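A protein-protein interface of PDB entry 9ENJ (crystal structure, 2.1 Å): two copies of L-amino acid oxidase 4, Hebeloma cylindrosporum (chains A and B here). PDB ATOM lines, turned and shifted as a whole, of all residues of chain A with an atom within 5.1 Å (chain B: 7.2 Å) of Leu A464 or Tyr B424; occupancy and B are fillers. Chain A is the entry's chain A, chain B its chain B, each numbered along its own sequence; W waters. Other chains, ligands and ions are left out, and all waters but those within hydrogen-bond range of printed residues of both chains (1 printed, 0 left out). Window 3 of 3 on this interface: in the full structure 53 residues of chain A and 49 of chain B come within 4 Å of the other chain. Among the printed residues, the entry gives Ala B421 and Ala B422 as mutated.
Water W1 lies within hydrogen-bond range of OG of Ser B415 (2.6 Å) and O of Met A466 (3.4 Å).
N of Leu A464 lies close to OD1 of Asn A462, 3.4 Å away.
The side-chain amide nitrogen of Asn A462 sits at hydrogen-bond distance from the side-chain hydroxyl of Thr A465, 3.2 Å away.
No position is printed for both chains.
Of the 6 pairs that touch across the chains among the printed residues, none has its exchanged pair printed and touching as well.
Of the 9 printed residues of chain A, 4 touch a printed residue of chain B.
Among the printed residues, 6 pairs touch across the chains.
Among the printed residues, no Asp or Glu carboxylate lies within 4 Å of a Lys or Arg side-chain nitrogen of the other chain.
Leu A464 touches one residue of chain B.
Tyr B424 touches just these residues of chain A: Pro A463 (3.4 Å) and Leu A464 (3.9 Å).
Printed residues of chain B within 4 Å of Asn A462: Ser B415 (3.0 Å).
Printed residues of chain B within 4 Å of Met A466: Ser B415 (3.5 Å).
The nearest residue of chain B that does not touch Leu A464 is Ser B415 (6.1 Å).
Among the printed residues, pairs that only touch across the chains: Pro A463 with Ser B415, Pro A463 with Tyr B424, Met A466 with Ser B415, Pro A463 with Leu B416 and Leu A464 with Tyr B424.
The side-chain hydroxyl (OG) of Ser B415 is in hydrogen-bond range of the backbone NH (N) of Asn A462 (3.0 Å).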
ATOM      1  N   ALA A  42     -26.297 -21.793   3.471  1.00  0.00           N
ATOM      2  CA  ALA A  42     -25.973 -22.654   2.338  1.00  0.00           C
ATOM      3  C   ALA A  42     -24.654 -23.383   2.547  1.00  0.00           C
ATOM      4  O   ALA A  42     -24.506 -24.540   2.137  1.00  0.00           O
ATOM      5  CB  ALA A  42     -25.919 -21.832   1.049  1.00  0.00           C
ATOM      6  N   SER A  43     -23.682 -22.729   3.173  1.00  0.00           N
ATOM      7  CA  SER A  43     -22.339 -23.274   3.265  1.00  0.00           C
ATOM      8  C   SER A  43     -22.175 -24.065   4.562  1.00  0.00           C
ATOM      9  O   SER A  43     -23.131 -24.293   5.309  1.00  0.00           O
ATOM     10  CB  SER A  43     -21.309 -22.151   3.174  1.00  0.00           C
ATOM     11  OG  SER A  43     -21.231 -21.442   4.400  1.00  0.00           O
ATOM     12  N   PRO A 315     -27.693 -11.812  -0.538  1.00  0.00           N
ATOM     13  CA  PRO A 315     -27.432 -10.728  -1.490  1.00  0.00           C
ATOM     14  C   PRO A 315     -28.486 -10.680  -2.585  1.00  0.00           C
ATOM     15  O   PRO A 315     -29.054 -11.702  -2.978  1.00  0.00           O
ATOM     16  CB  PRO A 315     -26.051 -11.077  -2.056  1.00  0.00           C
ATOM     17  CG  PRO A 315     -25.398 -11.871  -0.980  1.00  0.00           C
ATOM     18  CD  PRO A 315     -26.496 -12.644  -0.306  1.00  0.00           C
ATOM     19  N   VAL A 318     -28.221 -13.109  -5.409  1.00  0.00           N
ATOM     20  CA  VAL A 318     -28.573 -14.470  -5.017  1.00  0.00           C
ATOM     21  C   VAL A 318     -30.084 -14.650  -5.023  1.00  0.00           C
ATOM     22  O   VAL A 318     -30.594 -15.695  -5.443  1.00  0.00           O
ATOM     23  CB  VAL A 318     -27.968 -14.799  -3.639  1.00  0.00           C
ATOM     24  CG1 VAL A 318     -28.447 -16.162  -3.155  1.00  0.00           C
ATOM     25  CG2 VAL A 318     -26.450 -14.759  -3.706  1.00  0.00           C
ATOM     26  N   ASN A 462     -17.955 -15.816  -7.054  1.00  0.00           N
ATOM     27  CA  ASN A 462     -18.281 -16.555  -5.846  1.00  0.00           C
ATOM     28  C   ASN A 462     -19.796 -16.679  -5.770  1.00  0.00           C
ATOM     29  O   ASN A 462     -20.487 -15.676  -5.546  1.00  0.00           O
ATOM     30  CB  ASN A 462     -17.723 -15.835  -4.619  1.00  0.00           C
ATOM     31  CG  ASN A 462     -18.074 -16.531  -3.325  1.00  0.00           C
ATOM     32  OD1 ASN A 462     -18.448 -17.705  -3.316  1.00  0.00           O
ATOM     33  ND2 ASN A 462     -17.974 -15.803  -2.221  1.00  0.00           N
ATOM     34  N   PRO A 463     -20.356 -17.875  -5.967  1.00  0.00           N
ATOM     35  CA  PRO A 463     -21.823 -18.003  -5.980  1.00  0.00           C
ATOM     36  C   PRO A 463     -22.509 -17.499  -4.725  1.00  0.00           C
ATOM     37  O   PRO A 463     -23.691 -17.141  -4.790  1.00  0.00           O
ATOM     38  CB  PRO A 463     -22.037 -19.514  -6.154  1.00  0.00           C
ATOM     39  CG  PRO A 463     -20.814 -19.984  -6.854  1.00  0.00           C
ATOM     40  CD  PRO A 463     -19.689 -19.139  -6.333  1.00  0.00           C
ATOM     41  N   LEU A 464     -21.817 -17.452  -3.588  1.00  0.00           N
ATOM     42  CA  LEU A 464     -22.464 -17.071  -2.340  1.00  0.00           C
ATOM     43  C   LEU A 464     -22.578 -15.560  -2.169  1.00  0.00           C
ATOM     44  O   LEU A 464     -23.340 -15.108  -1.309  1.00  0.00           O
ATOM     45  CB  LEU A 464     -21.705 -17.677  -1.157  1.00  0.00           C
ATOM     46  CG  LEU A 464     -21.684 -19.206  -1.088  1.00  0.00           C
ATOM     47  CD1 LEU A 464     -20.770 -19.692   0.028  1.00  0.00           C
ATOM     48  CD2 LEU A 464     -23.093 -19.754  -0.897  1.00  0.00           C
ATOM     49  N   THR A 465     -21.844 -14.777  -2.957  1.00  0.00           N
ATOM     50  CA  THR A 465     -21.923 -13.321  -2.901  1.00  0.00           C
ATOM     51  C   THR A 465     -22.277 -12.690  -4.237  1.00  0.00           C
ATOM     52  O   THR A 465     -23.017 -11.701  -4.267  1.00  0.00           O
ATOM     53  CB  THR A 465     -20.595 -12.728  -2.398  1.00  0.00           C
ATOM     54  OG1 THR A 465     -19.520 -13.149  -3.247  1.00  0.00           O
ATOM     55  CG2 THR A 465     -20.320 -13.162  -0.969  1.00  0.00           C
ATOM     56  N   MET A 466     -21.771 -13.237  -5.342  1.00  0.00           N
ATOM     57  CA  MET A 466     -22.066 -12.734  -6.683  1.00  0.00           C
ATOM     58  C   MET A 466     -21.743 -11.245  -6.774  1.00  0.00           C
ATOM     59  O   MET A 466     -22.545 -10.426  -7.227  1.00  0.00           O
ATOM     60  CB  MET A 466     -23.521 -13.018  -7.055  1.00  0.00           C
ATOM     61  CG  MET A 466     -23.885 -14.497  -6.948  1.00  0.00           C
ATOM     62  SD  MET A 466     -25.560 -14.900  -7.478  1.00  0.00           S
ATOM     63  CE  MET A 466     -25.314 -15.171  -9.230  1.00  0.00           C
ATOM     64  N   SER B 415     -20.472 -15.583 -11.714  1.00  0.00           N
ATOM     65  CA  SER B 415     -20.115 -16.259 -10.473  1.00  0.00           C
ATOM     66  C   SER B 415     -20.554 -17.716 -10.464  1.00  0.00           C
ATOM     67  O   SER B 415     -20.007 -18.506  -9.689  1.00  0.00           O
ATOM     68  CB  SER B 415     -20.727 -15.536  -9.270  1.00  0.00           C
ATOM     69  OG  SER B 415     -19.912 -14.457  -8.851  1.00  0.00           O
ATOM     70  N   LEU B 416     -21.516 -18.086 -11.307  1.00  0.00           N
ATOM     71  CA  LEU B 416     -21.992 -19.457 -11.406  1.00  0.00           C
ATOM     72  C   LEU B 416     -21.310 -20.249 -12.515  1.00  0.00           C
ATOM     73  O   LEU B 416     -21.644 -21.420 -12.712  1.00  0.00           O
ATOM     74  CB  LEU B 416     -23.510 -19.475 -11.630  1.00  0.00           C
ATOM     75  CG  LEU B 416     -24.363 -18.941 -10.478  1.00  0.00           C
ATOM     76  CD1 LEU B 416     -25.843 -18.958 -10.841  1.00  0.00           C
ATOM     77  CD2 LEU B 416     -24.115 -19.746  -9.217  1.00  0.00           C
ATOM     78  N   ILE B 417     -20.369 -19.648 -13.238  1.00  0.00           N
ATOM     79  CA  ILE B 417     -19.715 -20.286 -14.374  1.00  0.00           C
ATOM     80  C   ILE B 417     -18.267 -20.584 -14.017  1.00  0.00           C
ATOM     81  O   ILE B 417     -17.595 -19.775 -13.369  1.00  0.00           O
ATOM     82  CB  ILE B 417     -19.803 -19.399 -15.632  1.00  0.00           C
ATOM     83  CG1 ILE B 417     -21.265 -19.266 -16.068  1.00  0.00           C
ATOM     84  CG2 ILE B 417     -18.932 -19.974 -16.747  1.00  0.00           C
ATOM     85  CD1 ILE B 417     -21.498 -18.252 -17.172  1.00  0.00           C
ATOM     86  N   THR B 419     -16.913 -22.705 -11.936  1.00  0.00           N
ATOM     87  CA  THR B 419     -16.576 -22.932 -10.538  1.00  0.00           C
ATOM     88  C   THR B 419     -15.830 -24.241 -10.313  1.00  0.00           C
ATOM     89  O   THR B 419     -15.126 -24.370  -9.307  1.00  0.00           O
ATOM     90  CB  THR B 419     -17.840 -22.935  -9.670  1.00  0.00           C
ATOM     91  OG1 THR B 419     -18.653 -24.068 -10.010  1.00  0.00           O
ATOM     92  CG2 THR B 419     -18.638 -21.650  -9.857  1.00  0.00           C
ATOM     93  N   GLY B 420     -15.967 -25.208 -11.217  1.00  0.00           N
ATOM     94  CA  GLY B 420     -15.379 -26.514 -11.015  1.00  0.00           C
ATOM     95  C   GLY B 420     -16.074 -27.371  -9.984  1.00  0.00           C
ATOM     96  O   GLY B 420     -15.601 -28.480  -9.706  1.00  0.00           O
ATOM     97  N   ALA B 421     -17.173 -26.897  -9.406  1.00  0.00           N
ATOM     98  CA  ALA B 421     -17.911 -27.620  -8.381  1.00  0.00           C
ATOM     99  C   ALA B 421     -19.215 -28.126  -8.980  1.00  0.00           C
ATOM    100  O   ALA B 421     -19.976 -27.349  -9.567  1.00  0.00           O
ATOM    101  CB  ALA B 421     -18.194 -26.725  -7.173  1.00  0.00           C
ATOM    102  N   ALA B 422     -19.469 -29.426  -8.828  1.00  0.00           N
ATOM    103  CA  ALA B 422     -20.687 -30.008  -9.380  1.00  0.00           C
ATOM    104  C   ALA B 422     -21.935 -29.349  -8.811  1.00  0.00           C
ATOM    105  O   ALA B 422     -22.938 -29.211  -9.520  1.00  0.00           O
ATOM    106  CB  ALA B 422     -20.715 -31.514  -9.107  1.00  0.00           C
ATOM    107  N   THR B 423     -21.894 -28.925  -7.547  1.00  0.00           N
ATOM    108  CA  THR B 423     -23.074 -28.323  -6.935  1.00  0.00           C
ATOM    109  C   THR B 423     -23.471 -27.033  -7.645  1.00  0.00           C
ATOM    110  O   THR B 423     -24.663 -26.762  -7.835  1.00  0.00           O
ATOM    111  CB  THR B 423     -22.822 -28.062  -5.449  1.00  0.00           C
ATOM    112  OG1 THR B 423     -24.004 -27.509  -4.856  1.00  0.00           O
ATOM    113  CG2 THR B 423     -21.656 -27.096  -5.250  1.00  0.00           C
ATOM    114  N   TYR B 424     -22.489 -26.225  -8.048  1.00  0.00           N
ATOM    115  CA  TYR B 424     -22.805 -24.979  -8.736  1.00  0.00           C
ATOM    116  C   TYR B 424     -23.122 -25.215 -10.206  1.00  0.00           C
ATOM    117  O   TYR B 424     -23.946 -24.492 -10.780  1.00  0.00           O
ATOM    118  CB  TYR B 424     -21.651 -23.992  -8.572  1.00  0.00           C
ATOM    119  CG  TYR B 424     -21.448 -23.556  -7.135  1.00  0.00           C
ATOM    120  CD1 TYR B 424     -22.522 -23.124  -6.363  1.00  0.00           C
ATOM    121  CD2 TYR B 424     -20.190 -23.583  -6.548  1.00  0.00           C
ATOM    122  CE1 TYR B 424     -22.349 -22.728  -5.050  1.00  0.00           C
ATOM    123  CE2 TYR B 424     -20.005 -23.186  -5.232  1.00  0.00           C
ATOM    124  CZ  TYR B 424     -21.088 -22.759  -4.490  1.00  0.00           C
ATOM    125  OH  TYR B 424     -20.916 -22.364  -3.183  1.00  0.00           O
ATOM    126  N   GLU B 425     -22.489 -26.211 -10.830  1.00  0.00           N
ATOM    127  CA  GLU B 425     -22.867 -26.592 -12.187  1.00  0.00           C
ATOM    128  C   GLU B 425     -24.331 -27.011 -12.242  1.00  0.00           C
ATOM    129  O   GLU B 425     -25.048 -26.683 -13.194  1.00  0.00           O
ATOM    130  CB  GLU B 425     -21.965 -27.726 -12.678  1.00  0.00           C
ATOM    131  CG  GLU B 425     -20.490 -27.359 -12.754  1.00  0.00           C
ATOM    132  CD  GLU B 425     -19.588 -28.568 -12.933  1.00  0.00           C
ATOM    133  OE1 GLU B 425     -20.047 -29.701 -12.679  1.00  0.00           O
ATOM    134  OE2 GLU B 425     -18.418 -28.384 -13.327  1.00  0.00           O
ATOM    135  N   GLU B 426     -24.790 -27.738 -11.219  1.00  0.00           N
ATOM    136  CA  GLU B 426     -26.194 -28.132 -11.152  1.00  0.00           C
ATOM    137  C   GLU B 426     -27.093 -26.926 -10.903  1.00  0.00           C
ATOM    138  O   GLU B 426     -28.156 -26.801 -11.521  1.00  0.00           O
ATOM    139  CB  GLU B 426     -26.385 -29.183 -10.059  1.00  0.00           C
ATOM    140  CG  GLU B 426     -25.707 -30.512 -10.361  1.00  0.00           C
ATOM    141  CD  GLU B 426     -25.784 -31.489  -9.201  1.00  0.00           C
ATOM    142  OE1 GLU B 426     -26.591 -31.255  -8.275  1.00  0.00           O
ATOM    143  OE2 GLU B 426     -25.038 -32.494  -9.219  1.00  0.00           O
ATOM    144  N   GLN B 427     -26.689 -26.030  -9.999  1.00  0.00           N
ATOM    145  CA  GLN B 427     -27.464 -24.814  -9.778  1.00  0.00           C
ATOM    146  C   GLN B 427     -27.584 -24.004 -11.064  1.00  0.00           C
ATOM    147  O   GLN B 427     -28.670 -23.523 -11.406  1.00  0.00           O
ATOM    148  CB  GLN B 427     -26.817 -23.966  -8.681  1.00  0.00           C
ATOM    149  CG  GLN B 427     -27.572 -22.678  -8.363  1.00  0.00           C
ATOM    150  CD  GLN B 427     -26.802 -21.757  -7.430  1.00  0.00           C
ATOM    151  OE1 GLN B 427     -25.740 -22.117  -6.919  1.00  0.00           O
ATOM    152  NE2 GLN B 427     -27.332 -20.558  -7.211  1.00  0.00           N
ATOM    153  N   LEU B 428     -26.475 -23.849 -11.793  1.00  0.00           N
ATOM    154  CA  LEU B 428     -26.504 -23.096 -13.042  1.00  0.00           C
ATOM    155  C   LEU B 428     -27.479 -23.712 -14.037  1.00  0.00           C
ATOM    156  O   LEU B 428     -28.307 -23.010 -14.628  1.00  0.00           O
ATOM    157  CB  LEU B 428     -25.099 -23.027 -13.639  1.00  0.00           C
ATOM    158  CG  LEU B 428     -24.971 -22.330 -14.996  1.00  0.00           C
ATOM    159  CD1 LEU B 428     -25.409 -20.880 -14.911  1.00  0.00           C
ATOM    160  CD2 LEU B 428     -23.541 -22.430 -15.503  1.00  0.00           C
ATOM    161  N   GLU B 429     -27.395 -25.029 -14.235  1.00  0.00           N
ATOM    162  CA  GLU B 429     -28.275 -25.688 -15.192  1.00  0.00           C
ATOM    163  C   GLU B 429     -29.737 -25.506 -14.807  1.00  0.00           C
ATOM    164  O   GLU B 429     -30.582 -25.203 -15.658  1.00  0.00           O
ATOM    165  CB  GLU B 429     -27.932 -27.177 -15.288  1.00  0.00           C
ATOM    166  CG  GLU B 429     -28.804 -27.938 -16.276  1.00  0.00           C
ATOM    167  CD  GLU B 429     -28.578 -29.433 -16.225  1.00  0.00           C
ATOM    168  OE1 GLU B 429     -27.436 -29.872 -16.473  1.00  0.00           O
ATOM    169  OE2 GLU B 429     -29.544 -30.164 -15.922  1.00  0.00           O
ATOM    170  N   HIS B 430     -30.058 -25.698 -13.526  1.00  0.00           N
ATOM    171  CA  HIS B 430     -31.446 -25.578 -13.096  1.00  0.00           C
ATOM    172  C   HIS B 430     -31.959 -24.156 -13.289  1.00  0.00           C
ATOM    173  O   HIS B 430     -33.112 -23.952 -13.684  1.00  0.00           O
ATOM    174  CB  HIS B 430     -31.587 -26.003 -11.635  1.00  0.00           C
ATOM    175  CG  HIS B 430     -32.997 -26.306 -11.235  1.00  0.00           C
ATOM    176  ND1 HIS B 430     -33.902 -25.327 -10.885  1.00  0.00           N
ATOM    177  CD2 HIS B 430     -33.659 -27.483 -11.136  1.00  0.00           C
ATOM    178  CE1 HIS B 430     -35.062 -25.888 -10.588  1.00  0.00           C
ATOM    179  NE2 HIS B 430     -34.940 -27.195 -10.731  1.00  0.00           N
HETATM  180  O   HOH W   1     -20.730 -12.101  -9.612  1.00  0.00           O
